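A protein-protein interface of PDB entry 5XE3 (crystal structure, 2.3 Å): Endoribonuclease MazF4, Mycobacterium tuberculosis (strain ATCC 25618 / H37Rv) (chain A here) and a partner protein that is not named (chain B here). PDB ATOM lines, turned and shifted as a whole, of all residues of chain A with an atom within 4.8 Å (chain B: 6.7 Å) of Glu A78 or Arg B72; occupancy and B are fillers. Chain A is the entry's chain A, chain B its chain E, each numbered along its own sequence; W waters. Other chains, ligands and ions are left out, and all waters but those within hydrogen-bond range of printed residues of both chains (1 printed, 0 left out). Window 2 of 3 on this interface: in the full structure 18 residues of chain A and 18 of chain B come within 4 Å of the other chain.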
ATOM      1  N   ARG A  13     -32.828  -9.435   5.915  1.00  0.00           N
ATOM      2  CA  ARG A  13     -33.582 -10.540   5.332  1.00  0.00           C
ATOM      3  C   ARG A  13     -32.728 -11.127   4.219  1.00  0.00           C
ATOM      4  O   ARG A  13     -32.070 -10.376   3.514  1.00  0.00           O
ATOM      5  CB  ARG A  13     -34.891 -10.020   4.742  1.00  0.00           C
ATOM      6  CG  ARG A  13     -35.867 -11.108   4.344  1.00  0.00           C
ATOM      7  CD  ARG A  13     -36.592 -11.682   5.549  1.00  0.00           C
ATOM      8  NE  ARG A  13     -37.493 -10.694   6.133  1.00  0.00           N
ATOM      9  CZ  ARG A  13     -38.314 -10.922   7.157  1.00  0.00           C
ATOM     10  NH1 ARG A  13     -38.373 -12.116   7.755  1.00  0.00           N
ATOM     11  NH2 ARG A  13     -39.077  -9.929   7.595  1.00  0.00           N
ATOM     12  N   CYS A  14     -32.720 -12.448   4.061  1.00  0.00           N
ATOM     13  CA  CYS A  14     -31.970 -13.080   2.954  1.00  0.00           C
ATOM     14  C   CYS A  14     -32.539 -14.463   2.641  1.00  0.00           C
ATOM     15  O   CYS A  14     -32.949 -15.209   3.546  1.00  0.00           O
ATOM     16  CB  CYS A  14     -30.453 -13.163   3.273  1.00  0.00           C
ATOM     17  SG  CYS A  14     -29.356 -13.659   1.879  1.00  0.00           S
ATOM     18  N   ASP A  15     -32.594 -14.779   1.351  1.00  0.00           N
ATOM     19  CA  ASP A  15     -33.030 -16.098   0.861  1.00  0.00           C
ATOM     20  C   ASP A  15     -31.818 -16.923   0.461  1.00  0.00           C
ATOM     21  O   ASP A  15     -31.190 -16.659  -0.561  1.00  0.00           O
ATOM     22  CB  ASP A  15     -33.947 -15.921  -0.370  1.00  0.00           C
ATOM     23  CG  ASP A  15     -34.674 -17.232  -0.774  1.00  0.00           C
ATOM     24  OD1 ASP A  15     -34.160 -18.347  -0.486  1.00  0.00           O
ATOM     25  OD2 ASP A  15     -35.784 -17.147  -1.370  1.00  0.00           O
ATOM     26  N   LEU A  16     -31.515 -17.952   1.231  1.00  0.00           N
ATOM     27  CA  LEU A  16     -30.412 -18.859   0.904  1.00  0.00           C
ATOM     28  C   LEU A  16     -30.782 -19.989  -0.025  1.00  0.00           C
ATOM     29  O   LEU A  16     -29.925 -20.787  -0.334  1.00  0.00           O
ATOM     30  CB  LEU A  16     -29.786 -19.446   2.174  1.00  0.00           C
ATOM     31  CG  LEU A  16     -28.589 -18.668   2.702  1.00  0.00           C
ATOM     32  CD1 LEU A  16     -28.913 -17.192   2.928  1.00  0.00           C
ATOM     33  CD2 LEU A  16     -28.112 -19.373   3.973  1.00  0.00           C
ATOM     34  N   THR A  73     -22.230 -17.704   5.446  1.00  0.00           N
ATOM     35  CA  THR A  73     -21.578 -16.622   4.681  1.00  0.00           C
ATOM     36  C   THR A  73     -22.525 -16.071   3.610  1.00  0.00           C
ATOM     37  O   THR A  73     -23.013 -16.845   2.783  1.00  0.00           O
ATOM     38  CB  THR A  73     -20.322 -17.134   4.006  1.00  0.00           C
ATOM     39  OG1 THR A  73     -19.507 -17.702   5.021  1.00  0.00           O
ATOM     40  CG2 THR A  73     -19.545 -16.005   3.299  1.00  0.00           C
ATOM     41  N   LEU A  74     -22.804 -14.756   3.662  1.00  0.00           N
ATOM     42  CA  LEU A  74     -23.792 -14.114   2.773  1.00  0.00           C
ATOM     43  C   LEU A  74     -23.137 -13.006   2.036  1.00  0.00           C
ATOM     44  O   LEU A  74     -22.505 -12.124   2.652  1.00  0.00           O
ATOM     45  CB  LEU A  74     -24.956 -13.457   3.541  1.00  0.00           C
ATOM     46  CG  LEU A  74     -25.572 -14.207   4.708  1.00  0.00           C
ATOM     47  CD1 LEU A  74     -26.633 -13.357   5.371  1.00  0.00           C
ATOM     48  CD2 LEU A  74     -26.156 -15.497   4.193  1.00  0.00           C
ATOM     49  N   GLY A  75     -23.369 -12.979   0.739  1.00  0.00           N
ATOM     50  CA  GLY A  75     -22.863 -11.905  -0.089  1.00  0.00           C
ATOM     51  C   GLY A  75     -23.535 -10.602   0.231  1.00  0.00           C
ATOM     52  O   GLY A  75     -24.740 -10.582   0.498  1.00  0.00           O
ATOM     53  N   LYS A  76     -22.772  -9.514   0.196  1.00  0.00           N
ATOM     54  CA  LYS A  76     -23.349  -8.180   0.399  1.00  0.00           C
ATOM     55  C   LYS A  76     -24.526  -7.968  -0.533  1.00  0.00           C
ATOM     56  O   LYS A  76     -25.588  -7.557  -0.075  1.00  0.00           O
ATOM     57  CB  LYS A  76     -22.293  -7.076   0.276  1.00  0.00           C
ATOM     58  CG  LYS A  76     -21.547  -6.837   1.594  1.00  0.00           C
ATOM     59  CD  LYS A  76     -20.166  -6.225   1.424  1.00  0.00           C
ATOM     60  CE  LYS A  76     -20.205  -4.781   0.990  1.00  0.00           C
ATOM     61  NZ  LYS A  76     -18.964  -4.420   0.248  1.00  0.00           N
ATOM     62  N   ASP A  77     -24.354  -8.327  -1.809  1.00  0.00           N
ATOM     63  CA  ASP A  77     -25.432  -8.249  -2.821  1.00  0.00           C
ATOM     64  C   ASP A  77     -26.681  -9.089  -2.531  1.00  0.00           C
ATOM     65  O   ASP A  77     -27.737  -8.846  -3.114  1.00  0.00           O
ATOM     66  CB  ASP A  77     -24.903  -8.603  -4.230  1.00  0.00           C
ATOM     67  CG  ASP A  77     -24.700 -10.131  -4.442  1.00  0.00           C
ATOM     68  OD1 ASP A  77     -23.840 -10.738  -3.721  1.00  0.00           O
ATOM     69  OD2 ASP A  77     -25.399 -10.707  -5.344  1.00  0.00           O
ATOM     70  N   GLU A  78     -26.563 -10.055  -1.656  1.00  0.00           N
ATOM     71  CA  GLU A  78     -27.653 -10.909  -1.327  1.00  0.00           C
ATOM     72  C   GLU A  78     -28.459 -10.385  -0.172  1.00  0.00           C
ATOM     73  O   GLU A  78     -29.524 -10.858   0.097  1.00  0.00           O
ATOM     74  CB  GLU A  78     -27.143 -12.259  -0.879  1.00  0.00           C
ATOM     75  CG  GLU A  78     -26.418 -13.121  -1.872  1.00  0.00           C
ATOM     76  CD  GLU A  78     -26.150 -14.514  -1.355  1.00  0.00           C
ATOM     77  OE1 GLU A  78     -25.088 -14.756  -0.812  1.00  0.00           O
ATOM     78  OE2 GLU A  78     -26.991 -15.376  -1.464  1.00  0.00           O
ATOM     79  N   LEU A  79     -27.931  -9.409   0.525  1.00  0.00           N
ATOM     80  CA  LEU A  79     -28.577  -8.915   1.713  1.00  0.00           C
ATOM     81  C   LEU A  79     -29.847  -8.146   2.004  1.00  0.00           C
ATOM     82  O   LEU A  79     -30.420  -8.326   3.051  1.00  0.00           O
ATOM     83  CB  LEU A  79     -27.734  -7.861   2.389  1.00  0.00           C
ATOM     84  CG  LEU A  79     -26.495  -8.430   3.039  1.00  0.00           C
ATOM     85  CD1 LEU A  79     -25.738  -7.365   3.758  1.00  0.00           C
ATOM     86  CD2 LEU A  79     -26.816  -9.572   3.956  1.00  0.00           C
ATOM     87  N   GLY A  80     -30.379  -7.420   1.091  1.00  0.00           N
ATOM     88  CA  GLY A  80     -31.710  -6.887   1.220  1.00  0.00           C
ATOM     89  C   GLY A  80     -32.294  -6.085   2.352  1.00  0.00           C
ATOM     90  O   GLY A  80     -31.701  -5.170   2.821  1.00  0.00           O
ATOM     91  N   SER B  67     -28.649 -28.811   2.297  1.00  0.00           N
ATOM     92  CA  SER B  67     -28.284 -28.949   0.892  1.00  0.00           C
ATOM     93  C   SER B  67     -27.935 -27.607   0.294  1.00  0.00           C
ATOM     94  O   SER B  67     -26.872 -27.440  -0.285  1.00  0.00           O
ATOM     95  CB  SER B  67     -29.432 -29.615   0.105  1.00  0.00           C
ATOM     96  OG  SER B  67     -29.567 -30.977   0.500  1.00  0.00           O
ATOM     97  N   ALA B  68     -28.839 -26.653   0.455  1.00  0.00           N
ATOM     98  CA  ALA B  68     -28.578 -25.297   0.056  1.00  0.00           C
ATOM     99  C   ALA B  68     -27.214 -24.815   0.599  1.00  0.00           C
ATOM    100  O   ALA B  68     -26.383 -24.364  -0.174  1.00  0.00           O
ATOM    101  CB  ALA B  68     -29.690 -24.405   0.531  1.00  0.00           C
ATOM    102  N   ALA B  69     -26.976 -25.000   1.907  1.00  0.00           N
ATOM    103  CA  ALA B  69     -25.735 -24.555   2.571  1.00  0.00           C
ATOM    104  C   ALA B  69     -24.496 -25.235   1.964  1.00  0.00           C
ATOM    105  O   ALA B  69     -23.491 -24.558   1.678  1.00  0.00           O
ATOM    106  CB  ALA B  69     -25.817 -24.816   4.069  1.00  0.00           C
ATOM    107  N   ARG B  70     -24.609 -26.537   1.693  1.00  0.00           N
ATOM    108  CA  ARG B  70     -23.546 -27.301   1.005  1.00  0.00           C
ATOM    109  C   ARG B  70     -23.246 -26.782  -0.395  1.00  0.00           C
ATOM    110  O   ARG B  70     -22.073 -26.590  -0.749  1.00  0.00           O
ATOM    111  CB  ARG B  70     -23.904 -28.776   0.854  1.00  0.00           C
ATOM    112  CG  ARG B  70     -24.010 -29.523   2.156  1.00  0.00           C
ATOM    113  CD  ARG B  70     -22.660 -29.815   2.765  1.00  0.00           C
ATOM    114  NE  ARG B  70     -22.842 -30.448   4.070  1.00  0.00           N
ATOM    115  CZ  ARG B  70     -23.224 -29.813   5.187  1.00  0.00           C
ATOM    116  NH1 ARG B  70     -23.494 -28.481   5.230  1.00  0.00           N
ATOM    117  NH2 ARG B  70     -23.356 -30.527   6.282  1.00  0.00           N
ATOM    118  N   ALA B  71     -24.305 -26.555  -1.179  1.00  0.00           N
ATOM    119  CA  ALA B  71     -24.157 -26.065  -2.558  1.00  0.00           C
ATOM    120  C   ALA B  71     -23.504 -24.719  -2.574  1.00  0.00           C
ATOM    121  O   ALA B  71     -22.669 -24.474  -3.420  1.00  0.00           O
ATOM    122  CB  ALA B  71     -25.500 -25.970  -3.272  1.00  0.00           C
ATOM    123  N   ARG B  72     -23.899 -23.834  -1.656  1.00  0.00           N
ATOM    124  CA  ARG B  72     -23.271 -22.504  -1.583  1.00  0.00           C
ATOM    125  C   ARG B  72     -21.783 -22.588  -1.142  1.00  0.00           C
ATOM    126  O   ARG B  72     -20.956 -21.798  -1.563  1.00  0.00           O
ATOM    127  CB  ARG B  72     -24.035 -21.603  -0.617  1.00  0.00           C
ATOM    128  CG  ARG B  72     -25.456 -21.293  -1.076  1.00  0.00           C
ATOM    129  CD  ARG B  72     -26.266 -20.552  -0.025  1.00  0.00           C
ATOM    130  NE  ARG B  72     -25.561 -19.359   0.423  1.00  0.00           N
ATOM    131  CZ  ARG B  72     -25.752 -18.120  -0.007  1.00  0.00           C
ATOM    132  NH1 ARG B  72     -26.658 -17.829  -0.944  1.00  0.00           N
ATOM    133  NH2 ARG B  72     -25.031 -17.157   0.511  1.00  0.00           N
ATOM    134  N   ARG B  73     -21.487 -23.515  -0.234  1.00  0.00           N
ATOM    135  CA  ARG B  73     -20.130 -23.742   0.187  1.00  0.00           C
ATOM    136  C   ARG B  73     -19.289 -24.205  -1.013  1.00  0.00           C
ATOM    137  O   ARG B  73     -18.237 -23.677  -1.244  1.00  0.00           O
ATOM    138  CB  ARG B  73     -20.113 -24.805   1.288  1.00  0.00           C
ATOM    139  CG  ARG B  73     -18.718 -25.244   1.724  1.00  0.00           C
ATOM    140  CD  ARG B  73     -18.784 -26.548   2.450  1.00  0.00           C
ATOM    141  NE  ARG B  73     -19.152 -27.616   1.543  1.00  0.00           N
ATOM    142  CZ  ARG B  73     -19.352 -28.880   1.896  1.00  0.00           C
ATOM    143  NH1 ARG B  73     -19.219 -29.269   3.162  1.00  0.00           N
ATOM    144  NH2 ARG B  73     -19.692 -29.755   0.968  1.00  0.00           N
ATOM    145  N   ASN B  74     -19.788 -25.184  -1.760  1.00  0.00           N
ATOM    146  CA  ASN B  74     -19.114 -25.720  -2.954  1.00  0.00           C
ATOM    147  C   ASN B  74     -18.892 -24.673  -4.025  1.00  0.00           C
ATOM    148  O   ASN B  74     -17.802 -24.567  -4.561  1.00  0.00           O
ATOM    149  CB  ASN B  74     -19.866 -26.913  -3.517  1.00  0.00           C
ATOM    150  CG  ASN B  74     -19.815 -28.123  -2.569  1.00  0.00           C
ATOM    151  OD1 ASN B  74     -19.044 -28.149  -1.613  1.00  0.00           O
ATOM    152  ND2 ASN B  74     -20.654 -29.109  -2.820  1.00  0.00           N
ATOM    153  N   ALA B  75     -19.892 -23.864  -4.287  1.00  0.00           N
ATOM    154  CA  ALA B  75     -19.716 -22.680  -5.129  1.00  0.00           C
ATOM    155  C   ALA B  75     -18.556 -21.785  -4.721  1.00  0.00           C
ATOM    156  O   ALA B  75     -17.841 -21.267  -5.584  1.00  0.00           O
ATOM    157  CB  ALA B  75     -21.014 -21.859  -5.151  1.00  0.00           C
ATOM    158  N   ARG B  76     -18.393 -21.577  -3.410  1.00  0.00           N
ATOM    159  CA  ARG B  76     -17.311 -20.752  -2.893  1.00  0.00           C
ATOM    160  C   ARG B  76     -15.930 -21.413  -3.069  1.00  0.00           C
ATOM    161  O   ARG B  76     -14.929 -20.706  -3.124  1.00  0.00           O
ATOM    162  CB  ARG B  76     -17.547 -20.384  -1.406  1.00  0.00           C
ATOM    163  CG  ARG B  76     -18.492 -19.204  -1.201  1.00  0.00           C
ATOM    164  CD  ARG B  76     -18.579 -18.743   0.255  1.00  0.00           C
ATOM    165  NE  ARG B  76     -19.030 -19.804   1.168  1.00  0.00           N
ATOM    166  CZ  ARG B  76     -20.297 -20.088   1.472  1.00  0.00           C
ATOM    167  NH1 ARG B  76     -21.324 -19.388   0.982  1.00  0.00           N
ATOM    168  NH2 ARG B  76     -20.546 -21.073   2.310  1.00  0.00           N
ATOM    169  N   GLN B  77     -15.878 -22.750  -3.089  1.00  0.00           N
ATOM    170  CA  GLN B  77     -14.611 -23.493  -3.203  1.00  0.00           C
ATOM    171  C   GLN B  77     -14.176 -23.494  -4.678  1.00  0.00           C
ATOM    172  O   GLN B  77     -13.024 -23.183  -4.998  1.00  0.00           O
ATOM    173  CB  GLN B  77     -14.755 -24.936  -2.669  1.00  0.00           C
ATOM    174  CG  GLN B  77     -15.177 -25.124  -1.203  1.00  0.00           C
ATOM    175  CD  GLN B  77     -14.377 -24.283  -0.193  1.00  0.00           C
ATOM    176  OE1 GLN B  77     -13.151 -24.438  -0.045  1.00  0.00           O
ATOM    177  NE2 GLN B  77     -15.070 -23.375   0.501  1.00  0.00           N
HETATM  178  O   HOH W   1     -23.621 -19.307   2.768  1.00  0.00           O
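Water W1 lies within hydrogen-bond range of the backbone carbonyl oxygen (O) of Thr A73 (2.5 Å), the guanidinium group (NH1) of Arg B76 (2.9 Å) and the guanidinium group (NE) of Arg B72 (3.0 Å).
Of the 12 printed residues of chain A, 4 touch a printed residue of chain B. Among the printed residues, 6 pairs touch across the chains. Among the printed residues, Asp or Glu carboxylates within 4 Å of a Lys or Arg side-chain nitrogen of the other chain: Glu A78 with Arg B72 (2.5 Å).
Among the printed residues, merely in contact across the chains: Thr A73 with Arg B76 (3.5 Å), Leu A16 with Arg B72 (3.7 Å), Leu A16 with Ala B68 (3.7 Å) and Leu A74 with Arg B72 (3.99 Å).
Of the printed residues of chain B, Leu A16 touches Ala B68 and Arg B72. Printed residues of chain B within 4 Å of Leu A74: Arg B72 (3.99 Å). Glu A78 touches one residue of chain B. Of the printed residues of chain A, Ala B68 touches Leu A16. Printed residues of chain A within 4 Å of Arg B72: Leu A16 (3.7 Å), Thr A73 (3.1 Å), Leu A74 (3.99 Å) and Glu A78 (2.5 Å). Of the printed residues of chain A, Arg B76 touches Thr A73. The nearest residue of chain B that does not touch Glu A78 is Arg B76 (6.2 Å). The nearest printed residue of chain A that does not touch Arg B72 is Gly A75 (4.5 Å).
The side-chain sulfur (SG) of Cys A14 lies within hydrogen-bond range of the backbone carbonyl oxygen (O) of Glu A78. The side-chain carboxylate of Glu A78 is in hydrogen-bond range of the backbone NH of Gly A75, at 2.9 Å.
NH1 of Arg B72 is in salt-bridge range of OE2 of Glu A78 (2.5 Å). NH2 of Arg B72 lies within hydrogen-bond range of O of Thr A73 (3.1 Å).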
